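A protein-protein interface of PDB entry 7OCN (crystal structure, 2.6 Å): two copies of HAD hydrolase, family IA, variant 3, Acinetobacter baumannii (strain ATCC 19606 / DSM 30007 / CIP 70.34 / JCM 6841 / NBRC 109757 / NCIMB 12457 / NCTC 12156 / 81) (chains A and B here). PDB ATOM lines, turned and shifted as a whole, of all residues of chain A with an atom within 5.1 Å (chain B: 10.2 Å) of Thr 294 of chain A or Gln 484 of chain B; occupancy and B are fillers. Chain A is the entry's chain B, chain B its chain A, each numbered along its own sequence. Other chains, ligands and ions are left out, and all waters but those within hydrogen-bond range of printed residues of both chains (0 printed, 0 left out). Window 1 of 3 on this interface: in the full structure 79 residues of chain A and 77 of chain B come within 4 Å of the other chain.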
ATOM      1  N   VAL A 289     -16.875  -5.650 -23.854  1.00  0.00           N
ATOM      2  CA  VAL A 289     -16.038  -5.243 -22.684  1.00  0.00           C
ATOM      3  C   VAL A 289     -16.378  -3.794 -22.309  1.00  0.00           C
ATOM      4  O   VAL A 289     -16.606  -3.539 -21.112  1.00  0.00           O
ATOM      5  CB  VAL A 289     -14.532  -5.405 -22.973  1.00  0.00           C
ATOM      6  CG1 VAL A 289     -13.673  -4.793 -21.875  1.00  0.00           C
ATOM      7  CG2 VAL A 289     -14.148  -6.860 -23.194  1.00  0.00           C
ATOM      8  N   PHE A 292     -19.926  -3.528 -20.656  1.00  0.00           N
ATOM      9  CA  PHE A 292     -19.929  -4.106 -19.283  1.00  0.00           C
ATOM     10  C   PHE A 292     -19.017  -3.287 -18.362  1.00  0.00           C
ATOM     11  O   PHE A 292     -19.357  -3.133 -17.173  1.00  0.00           O
ATOM     12  CB  PHE A 292     -19.488  -5.573 -19.298  1.00  0.00           C
ATOM     13  CG  PHE A 292     -20.617  -6.570 -19.356  1.00  0.00           C
ATOM     14  CD1 PHE A 292     -21.170  -6.952 -20.569  1.00  0.00           C
ATOM     15  CD2 PHE A 292     -21.126  -7.130 -18.194  1.00  0.00           C
ATOM     16  CE1 PHE A 292     -22.209  -7.870 -20.617  1.00  0.00           C
ATOM     17  CE2 PHE A 292     -22.164  -8.048 -18.243  1.00  0.00           C
ATOM     18  CZ  PHE A 292     -22.703  -8.417 -19.455  1.00  0.00           C
ATOM     19  N   GLY A 293     -17.889  -2.801 -18.893  1.00  0.00           N
ATOM     20  CA  GLY A 293     -16.857  -2.060 -18.141  1.00  0.00           C
ATOM     21  C   GLY A 293     -15.718  -2.969 -17.713  1.00  0.00           C
ATOM     22  O   GLY A 293     -14.570  -2.488 -17.648  1.00  0.00           O
ATOM     23  N   THR A 294     -16.025  -4.239 -17.429  1.00  0.00           N
ATOM     24  CA  THR A 294     -15.055  -5.288 -17.021  1.00  0.00           C
ATOM     25  C   THR A 294     -15.272  -6.547 -17.866  1.00  0.00           C
ATOM     26  O   THR A 294     -16.340  -6.662 -18.503  1.00  0.00           O
ATOM     27  CB  THR A 294     -15.193  -5.613 -15.528  1.00  0.00           C
ATOM     28  OG1 THR A 294     -16.482  -6.193 -15.322  1.00  0.00           O
ATOM     29  CG2 THR A 294     -15.031  -4.399 -14.641  1.00  0.00           C
ATOM     30  N   TYR A 295     -14.279  -7.441 -17.872  1.00  0.00           N
ATOM     31  CA  TYR A 295     -14.375  -8.837 -18.371  1.00  0.00           C
ATOM     32  C   TYR A 295     -13.626  -9.741 -17.388  1.00  0.00           C
ATOM     33  O   TYR A 295     -12.751  -9.229 -16.661  1.00  0.00           O
ATOM     34  CB  TYR A 295     -13.833  -8.952 -19.799  1.00  0.00           C
ATOM     35  CG  TYR A 295     -12.330  -9.007 -19.904  1.00  0.00           C
ATOM     36  CD1 TYR A 295     -11.649 -10.211 -19.810  1.00  0.00           C
ATOM     37  CD2 TYR A 295     -11.584  -7.855 -20.096  1.00  0.00           C
ATOM     38  CE1 TYR A 295     -10.268 -10.270 -19.900  1.00  0.00           C
ATOM     39  CE2 TYR A 295     -10.203  -7.897 -20.192  1.00  0.00           C
ATOM     40  CZ  TYR A 295      -9.542  -9.108 -20.092  1.00  0.00           C
ATOM     41  OH  TYR A 295      -8.182  -9.147 -20.184  1.00  0.00           O
ATOM     42  N   SER A 296     -13.959 -11.034 -17.369  1.00  0.00           N
ATOM     43  CA  SER A 296     -13.413 -12.031 -16.411  1.00  0.00           C
ATOM     44  C   SER A 296     -12.714 -13.169 -17.162  1.00  0.00           C
ATOM     45  O   SER A 296     -13.208 -13.563 -18.238  1.00  0.00           O
ATOM     46  CB  SER A 296     -14.497 -12.551 -15.506  1.00  0.00           C
ATOM     47  OG  SER A 296     -15.122 -11.488 -14.801  1.00  0.00           O
ATOM     48  N   ARG A 307     -12.201 -11.158 -12.301  1.00  0.00           N
ATOM     49  CA  ARG A 307     -12.648  -9.865 -12.887  1.00  0.00           C
ATOM     50  C   ARG A 307     -11.425  -8.969 -13.111  1.00  0.00           C
ATOM     51  O   ARG A 307     -10.616  -8.827 -12.171  1.00  0.00           O
ATOM     52  CB  ARG A 307     -13.678  -9.179 -11.983  1.00  0.00           C
ATOM     53  CG  ARG A 307     -14.224  -7.874 -12.545  1.00  0.00           C
ATOM     54  CD  ARG A 307     -15.240  -7.199 -11.641  1.00  0.00           C
ATOM     55  NE  ARG A 307     -16.583  -7.750 -11.794  1.00  0.00           N
ATOM     56  CZ  ARG A 307     -17.114  -8.719 -11.051  1.00  0.00           C
ATOM     57  NH1 ARG A 307     -18.350  -9.126 -11.294  1.00  0.00           N
ATOM     58  NH2 ARG A 307     -16.425  -9.284 -10.072  1.00  0.00           N
ATOM     59  N   ILE A 308     -11.303  -8.396 -14.313  1.00  0.00           N
ATOM     60  CA  ILE A 308     -10.216  -7.452 -14.708  1.00  0.00           C
ATOM     61  C   ILE A 308     -10.861  -6.117 -15.096  1.00  0.00           C
ATOM     62  O   ILE A 308     -11.607  -6.090 -16.095  1.00  0.00           O
ATOM     63  CB  ILE A 308      -9.359  -8.049 -15.843  1.00  0.00           C
ATOM     64  CG1 ILE A 308      -8.606  -9.295 -15.369  1.00  0.00           C
ATOM     65  CG2 ILE A 308      -8.413  -7.003 -16.418  1.00  0.00           C
ATOM     66  CD1 ILE A 308      -8.072 -10.158 -16.482  1.00  0.00           C
ATOM     67  N   GLU A 309     -10.565  -5.059 -14.336  1.00  0.00           N
ATOM     68  CA  GLU A 309     -11.221  -3.727 -14.441  1.00  0.00           C
ATOM     69  C   GLU A 309     -10.195  -2.688 -14.907  1.00  0.00           C
ATOM     70  O   GLU A 309      -8.993  -3.023 -14.971  1.00  0.00           O
ATOM     71  CB  GLU A 309     -11.890  -3.349 -13.114  1.00  0.00           C
ATOM     72  CG  GLU A 309     -10.965  -3.371 -11.904  1.00  0.00           C
ATOM     73  CD  GLU A 309     -11.671  -3.420 -10.557  1.00  0.00           C
ATOM     74  OE1 GLU A 309     -12.757  -4.029 -10.476  1.00  0.00           O
ATOM     75  OE2 GLU A 309     -11.131  -2.851  -9.587  1.00  0.00           O
ATOM     76  N   ASN A 310     -10.670  -1.481 -15.237  1.00  0.00           N
ATOM     77  CA  ASN A 310      -9.871  -0.366 -15.817  1.00  0.00           C
ATOM     78  C   ASN A 310      -9.430  -0.750 -17.235  1.00  0.00           C
ATOM     79  O   ASN A 310      -8.323  -0.340 -17.640  1.00  0.00           O
ATOM     80  CB  ASN A 310      -8.670  -0.004 -14.939  1.00  0.00           C
ATOM     81  CG  ASN A 310      -9.032   0.179 -13.480  1.00  0.00           C
ATOM     82  OD1 ASN A 310     -10.059   0.773 -13.160  1.00  0.00           O
ATOM     83  ND2 ASN A 310      -8.190  -0.324 -12.591  1.00  0.00           N
ATOM     84  N   LEU A 488     -18.743 -10.986 -17.382  1.00  0.00           N
ATOM     85  CA  LEU A 488     -18.502 -11.226 -18.832  1.00  0.00           C
ATOM     86  C   LEU A 488     -17.302 -12.169 -18.985  1.00  0.00           C
ATOM     87  O   LEU A 488     -16.158 -11.705 -18.815  1.00  0.00           O
ATOM     88  CB  LEU A 488     -18.259  -9.886 -19.534  1.00  0.00           C
ATOM     89  CG  LEU A 488     -18.115  -9.951 -21.055  1.00  0.00           C
ATOM     90  CD1 LEU A 488     -19.444 -10.286 -21.714  1.00  0.00           C
ATOM     91  CD2 LEU A 488     -17.564  -8.645 -21.606  1.00  0.00           C
ATOM     92  N   PHE B 292     -26.309   2.680  -3.952  1.00  0.00           N
ATOM     93  CA  PHE B 292     -25.010   2.103  -4.398  1.00  0.00           C
ATOM     94  C   PHE B 292     -25.150   0.592  -4.617  1.00  0.00           C
ATOM     95  O   PHE B 292     -24.408   0.042  -5.455  1.00  0.00           O
ATOM     96  CB  PHE B 292     -23.898   2.395  -3.384  1.00  0.00           C
ATOM     97  CG  PHE B 292     -23.040   3.591  -3.710  1.00  0.00           C
ATOM     98  CD1 PHE B 292     -23.436   4.872  -3.356  1.00  0.00           C
ATOM     99  CD2 PHE B 292     -21.828   3.434  -4.367  1.00  0.00           C
ATOM    100  CE1 PHE B 292     -22.641   5.968  -3.656  1.00  0.00           C
ATOM    101  CE2 PHE B 292     -21.035   4.531  -4.666  1.00  0.00           C
ATOM    102  CZ  PHE B 292     -21.443   5.796  -4.310  1.00  0.00           C
ATOM    103  N   THR B 294     -24.412  -1.525  -2.321  1.00  0.00           N
ATOM    104  CA  THR B 294     -23.222  -2.027  -1.581  1.00  0.00           C
ATOM    105  C   THR B 294     -22.616  -0.882  -0.761  1.00  0.00           C
ATOM    106  O   THR B 294     -22.725   0.277  -1.203  1.00  0.00           O
ATOM    107  CB  THR B 294     -22.182  -2.618  -2.542  1.00  0.00           C
ATOM    108  OG1 THR B 294     -21.049  -3.026  -1.776  1.00  0.00           O
ATOM    109  CG2 THR B 294     -21.743  -1.648  -3.617  1.00  0.00           C
ATOM    110  N   SER B 296     -18.891  -0.272   2.105  1.00  0.00           N
ATOM    111  CA  SER B 296     -17.496  -0.736   2.324  1.00  0.00           C
ATOM    112  C   SER B 296     -17.035  -0.425   3.754  1.00  0.00           C
ATOM    113  O   SER B 296     -17.442   0.620   4.298  1.00  0.00           O
ATOM    114  CB  SER B 296     -16.574  -0.133   1.298  1.00  0.00           C
ATOM    115  OG  SER B 296     -16.883  -0.620   0.001  1.00  0.00           O
ATOM    116  N   ASP B 305     -10.105  -1.176   1.924  1.00  0.00           N
ATOM    117  CA  ASP B 305     -11.572  -0.951   1.813  1.00  0.00           C
ATOM    118  C   ASP B 305     -12.241  -2.267   1.394  1.00  0.00           C
ATOM    119  O   ASP B 305     -12.014  -2.709   0.251  1.00  0.00           O
ATOM    120  CB  ASP B 305     -11.884   0.186   0.837  1.00  0.00           C
ATOM    121  CG  ASP B 305     -11.382   1.545   1.297  1.00  0.00           C
ATOM    122  OD1 ASP B 305     -10.863   1.631   2.428  1.00  0.00           O
ATOM    123  OD2 ASP B 305     -11.516   2.510   0.519  1.00  0.00           O
ATOM    124  N   ARG B 307     -15.352  -4.472   0.381  1.00  0.00           N
ATOM    125  CA  ARG B 307     -16.662  -4.345  -0.314  1.00  0.00           C
ATOM    126  C   ARG B 307     -17.621  -5.421   0.210  1.00  0.00           C
ATOM    127  O   ARG B 307     -17.376  -6.612  -0.064  1.00  0.00           O
ATOM    128  CB  ARG B 307     -16.470  -4.473  -1.830  1.00  0.00           C
ATOM    129  CG  ARG B 307     -17.743  -4.294  -2.649  1.00  0.00           C
ATOM    130  CD  ARG B 307     -17.946  -2.870  -3.129  1.00  0.00           C
ATOM    131  NE  ARG B 307     -16.986  -2.498  -4.160  1.00  0.00           N
ATOM    132  CZ  ARG B 307     -16.969  -1.334  -4.804  1.00  0.00           C
ATOM    133  NH1 ARG B 307     -16.045  -1.104  -5.724  1.00  0.00           N
ATOM    134  NH2 ARG B 307     -17.868  -0.403  -4.535  1.00  0.00           N
ATOM    135  N   HIS B 440     -18.247  11.772 -14.654  1.00  0.00           N
ATOM    136  CA  HIS B 440     -18.283  10.488 -15.406  1.00  0.00           C
ATOM    137  C   HIS B 440     -19.383  10.533 -16.477  1.00  0.00           C
ATOM    138  O   HIS B 440     -19.167   9.952 -17.555  1.00  0.00           O
ATOM    139  CB  HIS B 440     -18.467   9.309 -14.440  1.00  0.00           C
ATOM    140  CG  HIS B 440     -18.565   7.983 -15.116  1.00  0.00           C
ATOM    141  ND1 HIS B 440     -17.477   7.377 -15.712  1.00  0.00           N
ATOM    142  CD2 HIS B 440     -19.610   7.146 -15.291  1.00  0.00           C
ATOM    143  CE1 HIS B 440     -17.848   6.223 -16.227  1.00  0.00           C
ATOM    144  NE2 HIS B 440     -19.151   6.058 -15.983  1.00  0.00           N
ATOM    145  N   MET B 473     -27.328  -2.826 -22.928  1.00  0.00           N
ATOM    146  CA  MET B 473     -26.379  -3.072 -21.807  1.00  0.00           C
ATOM    147  C   MET B 473     -25.529  -1.820 -21.559  1.00  0.00           C
ATOM    148  O   MET B 473     -25.409  -1.415 -20.386  1.00  0.00           O
ATOM    149  CB  MET B 473     -25.457  -4.255 -22.114  1.00  0.00           C
ATOM    150  CG  MET B 473     -26.143  -5.601 -22.008  1.00  0.00           C
ATOM    151  SD  MET B 473     -25.106  -6.951 -22.620  1.00  0.00           S
ATOM    152  CE  MET B 473     -25.950  -8.360 -21.903  1.00  0.00           C
ATOM    153  N   PHE B 477     -25.444   0.064 -17.965  1.00  0.00           N
ATOM    154  CA  PHE B 477     -24.237  -0.285 -17.165  1.00  0.00           C
ATOM    155  C   PHE B 477     -23.239   0.881 -17.128  1.00  0.00           C
ATOM    156  O   PHE B 477     -22.668   1.122 -16.045  1.00  0.00           O
ATOM    157  CB  PHE B 477     -23.555  -1.544 -17.713  1.00  0.00           C
ATOM    158  CG  PHE B 477     -24.377  -2.809 -17.669  1.00  0.00           C
ATOM    159  CD1 PHE B 477     -25.258  -3.062 -16.627  1.00  0.00           C
ATOM    160  CD2 PHE B 477     -24.241  -3.769 -18.660  1.00  0.00           C
ATOM    161  CE1 PHE B 477     -26.001  -4.232 -16.592  1.00  0.00           C
ATOM    162  CE2 PHE B 477     -24.983  -4.940 -18.623  1.00  0.00           C
ATOM    163  CZ  PHE B 477     -25.862  -5.171 -17.590  1.00  0.00           C
ATOM    164  N   GLN B 478     -23.035   1.572 -18.258  1.00  0.00           N
ATOM    165  CA  GLN B 478     -21.966   2.597 -18.441  1.00  0.00           C
ATOM    166  C   GLN B 478     -22.021   3.636 -17.321  1.00  0.00           C
ATOM    167  O   GLN B 478     -20.976   3.995 -16.783  1.00  0.00           O
ATOM    168  CB  GLN B 478     -22.048   3.249 -19.825  1.00  0.00           C
ATOM    169  CG  GLN B 478     -20.916   4.228 -20.107  1.00  0.00           C
ATOM    170  CD  GLN B 478     -20.806   4.585 -21.571  1.00  0.00           C
ATOM    171  OE1 GLN B 478     -21.751   4.433 -22.343  1.00  0.00           O
ATOM    172  NE2 GLN B 478     -19.641   5.071 -21.965  1.00  0.00           N
ATOM    173  N   PRO B 479     -23.208   4.163 -16.930  1.00  0.00           N
ATOM    174  CA  PRO B 479     -23.291   5.105 -15.810  1.00  0.00           C
ATOM    175  C   PRO B 479     -22.747   4.557 -14.480  1.00  0.00           C
ATOM    176  O   PRO B 479     -22.305   5.353 -13.671  1.00  0.00           O
ATOM    177  CB  PRO B 479     -24.796   5.393 -15.687  1.00  0.00           C
ATOM    178  CG  PRO B 479     -25.342   5.102 -17.067  1.00  0.00           C
ATOM    179  CD  PRO B 479     -24.519   3.930 -17.556  1.00  0.00           C
ATOM    180  N   GLY B 480     -22.792   3.231 -14.290  1.00  0.00           N
ATOM    181  CA  GLY B 480     -22.352   2.539 -13.061  1.00  0.00           C
ATOM    182  C   GLY B 480     -20.942   1.973 -13.160  1.00  0.00           C
ATOM    183  O   GLY B 480     -20.556   1.224 -12.243  1.00  0.00           O
ATOM    184  N   HIS B 481     -20.195   2.312 -14.217  1.00  0.00           N
ATOM    185  CA  HIS B 481     -18.779   1.898 -14.430  1.00  0.00           C
ATOM    186  C   HIS B 481     -17.881   2.490 -13.336  1.00  0.00           C
ATOM    187  O   HIS B 481     -16.857   1.856 -13.015  1.00  0.00           O
ATOM    188  CB  HIS B 481     -18.294   2.311 -15.828  1.00  0.00           C
ATOM    189  CG  HIS B 481     -18.732   1.389 -16.916  1.00  0.00           C
ATOM    190  ND1 HIS B 481     -19.784   0.510 -16.756  1.00  0.00           N
ATOM    191  CD2 HIS B 481     -18.280   1.217 -18.176  1.00  0.00           C
ATOM    192  CE1 HIS B 481     -19.954  -0.174 -17.867  1.00  0.00           C
ATOM    193  NE2 HIS B 481     -19.045   0.243 -18.757  1.00  0.00           N
ATOM    194  N   ILE B 482     -18.249   3.657 -12.798  1.00  0.00           N
ATOM    195  CA  ILE B 482     -17.475   4.407 -11.763  1.00  0.00           C
ATOM    196  C   ILE B 482     -17.396   3.575 -10.472  1.00  0.00           C
ATOM    197  O   ILE B 482     -16.419   3.757  -9.722  1.00  0.00           O
ATOM    198  CB  ILE B 482     -18.084   5.808 -11.532  1.00  0.00           C
ATOM    199  CG1 ILE B 482     -17.099   6.763 -10.850  1.00  0.00           C
ATOM    200  CG2 ILE B 482     -19.402   5.723 -10.773  1.00  0.00           C
ATOM    201  CD1 ILE B 482     -16.015   7.288 -11.764  1.00  0.00           C
ATOM    202  N   LEU B 483     -18.368   2.683 -10.237  1.00  0.00           N
ATOM    203  CA  LEU B 483     -18.446   1.814  -9.027  1.00  0.00           C
ATOM    204  C   LEU B 483     -17.275   0.821  -8.989  1.00  0.00           C
ATOM    205  O   LEU B 483     -17.032   0.262  -7.900  1.00  0.00           O
ATOM    206  CB  LEU B 483     -19.786   1.067  -9.015  1.00  0.00           C
ATOM    207  CG  LEU B 483     -21.035   1.934  -8.855  1.00  0.00           C
ATOM    208  CD1 LEU B 483     -22.295   1.093  -8.994  1.00  0.00           C
ATOM    209  CD2 LEU B 483     -21.028   2.665  -7.520  1.00  0.00           C
ATOM    210  N   GLN B 484     -16.598   0.591 -10.122  1.00  0.00           N
ATOM    211  CA  GLN B 484     -15.386  -0.271 -10.229  1.00  0.00           C
ATOM    212  C   GLN B 484     -14.349   0.171  -9.187  1.00  0.00           C
ATOM    213  O   GLN B 484     -13.915  -0.685  -8.386  1.00  0.00           O
ATOM    214  CB  GLN B 484     -14.777  -0.194 -11.632  1.00  0.00           C
ATOM    215  CG  GLN B 484     -15.532  -1.002 -12.680  1.00  0.00           C
ATOM    216  CD  GLN B 484     -14.965  -0.823 -14.069  1.00  0.00           C
ATOM    217  OE1 GLN B 484     -13.780  -0.549 -14.251  1.00  0.00           O
ATOM    218  NE2 GLN B 484     -15.816  -0.984 -15.069  1.00  0.00           N
ATOM    219  N   SER B 485     -13.975   1.454  -9.213  1.00  0.00           N
ATOM    220  CA  SER B 485     -12.992   2.097  -8.300  1.00  0.00           C
ATOM    221  C   SER B 485     -13.678   3.233  -7.531  1.00  0.00           C
ATOM    222  O   SER B 485     -13.281   4.404  -7.714  1.00  0.00           O
ATOM    223  CB  SER B 485     -11.789   2.586  -9.071  1.00  0.00           C
ATOM    224  OG  SER B 485     -10.895   3.303  -8.229  1.00  0.00           O
ATOM    225  N   MET B 486     -14.680   2.891  -6.714  1.00  0.00           N
ATOM    226  CA  MET B 486     -15.451   3.842  -5.868  1.00  0.00           C
ATOM    227  C   MET B 486     -16.192   3.056  -4.782  1.00  0.00           C
ATOM    228  O   MET B 486     -17.064   2.238  -5.141  1.00  0.00           O
ATOM    229  CB  MET B 486     -16.460   4.634  -6.705  1.00  0.00           C
ATOM    230  CG  MET B 486     -17.238   5.665  -5.905  1.00  0.00           C
ATOM    231  SD  MET B 486     -18.133   6.841  -6.953  1.00  0.00           S
ATOM    232  CE  MET B 486     -16.772   7.820  -7.584  1.00  0.00           C
ATOM    233  N   ASP B 487     -15.856   3.303  -3.512  1.00  0.00           N
ATOM    234  CA  ASP B 487     -16.389   2.570  -2.333  1.00  0.00           C
ATOM    235  C   ASP B 487     -17.136   3.547  -1.419  1.00  0.00           C
ATOM    236  O   ASP B 487     -16.542   4.577  -1.041  1.00  0.00           O
ATOM    237  CB  ASP B 487     -15.264   1.855  -1.582  1.00  0.00           C
ATOM    238  CG  ASP B 487     -14.678   0.681  -2.347  1.00  0.00           C
ATOM    239  OD1 ASP B 487     -14.141   0.912  -3.449  1.00  0.00           O
ATOM    240  OD2 ASP B 487     -14.771  -0.455  -1.839  1.00  0.00           O
ATOM    241  N   LEU B 488     -18.390   3.227  -1.081  1.00  0.00           N
ATOM    242  CA  LEU B 488     -19.220   3.980  -0.101  1.00  0.00           C
ATOM    243  C   LEU B 488     -18.812   3.552   1.314  1.00  0.00           C
ATOM    244  O   LEU B 488     -19.372   2.560   1.821  1.00  0.00           O
ATOM    245  CB  LEU B 488     -20.703   3.702  -0.377  1.00  0.00           C
ATOM    246  CG  LEU B 488     -21.696   4.506   0.462  1.00  0.00           C
ATOM    247  CD1 LEU B 488     -21.669   5.977   0.079  1.00  0.00           C
ATOM    248  CD2 LEU B 488     -23.103   3.947   0.316  1.00  0.00           C
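CE1 of Phe 292 of chain A touches SD of Met 473 of chain B, 3.6 Å away. Phe 292 of chain A touches His 481 of chain B (O to CE1, 3.1 Å). Thr 294 of chain A touches Gln 484 of chain B (CG2 to NE2, 3.5 Å). CB of Glu 309 of chain A touches OE1 of Gln 484 of chain B, at 3.6 Å.
The backbone carbonyl oxygen (O) of Phe 477 of chain B lies within hydrogen-bond range of a ring nitrogen (ND1) of His 481 of chain B, 3.0 Å away. The guanidinium group of Arg 307 of chain B is in hydrogen-bond range of the backbone carbonyl oxygen of Gln 484 of chain B (3.4 Å).
Of the 19 printed residues of chain B, 3 touch a printed residue of chain A. Printed residues of chain B that touch a printed residue of chain A: Met 473, His 481 and Gln 484. Hydrophobic or aromatic side chains of chain B that line the printed part of chain A: Met 473 and His 481. Hydrophobic or aromatic side chains of chain A within 4 Å of the printed part of chain B: Phe 292. Along chain A the printed residues that touch a printed residue of chain B span positions 292 to 310. Among the printed residues, no Asp or Glu carboxylate lies within 4 Å of a Lys or Arg side-chain nitrogen of the other chain.
The side-chain amide nitrogen of Gln 484 of chain B lies within hydrogen-bond range of the backbone carbonyl oxygen of Gly 293 of chain A (3.2 Å). A ring nitrogen (NE2) of His 481 of chain B lies close to the backbone NH (N) of Gly 293 of chain A. The side-chain amide oxygen (OE1) of Gln 484 of chain B is in hydrogen-bond range of the backbone NH (N) of Asn 310 of chain A, 3.4 Å away.
Of the printed residues of chain B, Phe 292 of chain A touches Met 473 (3.6 Å) and His 481 (3.1 Å). Gly 293 of chain A touches just these residues of chain B: His 481 (3.2 Å) and Gln 484 (3.2 Å). Printed residues of chain B within 4 Å of Thr 294 of chain A: Gln 484 (3.5 Å). Of chain B, only Gln 484 comes within 4 Å of Glu 309 of chain A. Of the printed residues of chain B, Asn 310 of chain A touches Gln 484 (3.4 Å). Of the printed residues of chain A, His 481 of chain B touches Phe 292 (3.1 Å) and Gly 293 (3.2 Å). Gln 484 of chain B touches four residues of chain A. Ser 485 of chain B touches none of the printed residues of chain A. The nearest residue of chain B that does not touch Thr 294 of chain A is His 481 of chain B (5.6 Å). The nearest residue of chain A that does not touch Gln 484 of chain B is Phe 292 of chain A (4.6 Å).
Positions printed for both chains: 292, 294, 296, 307 and 488. Of the 7 pairs that touch across the chains among the printed residues, none has its exchanged pair printed and touching as well.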
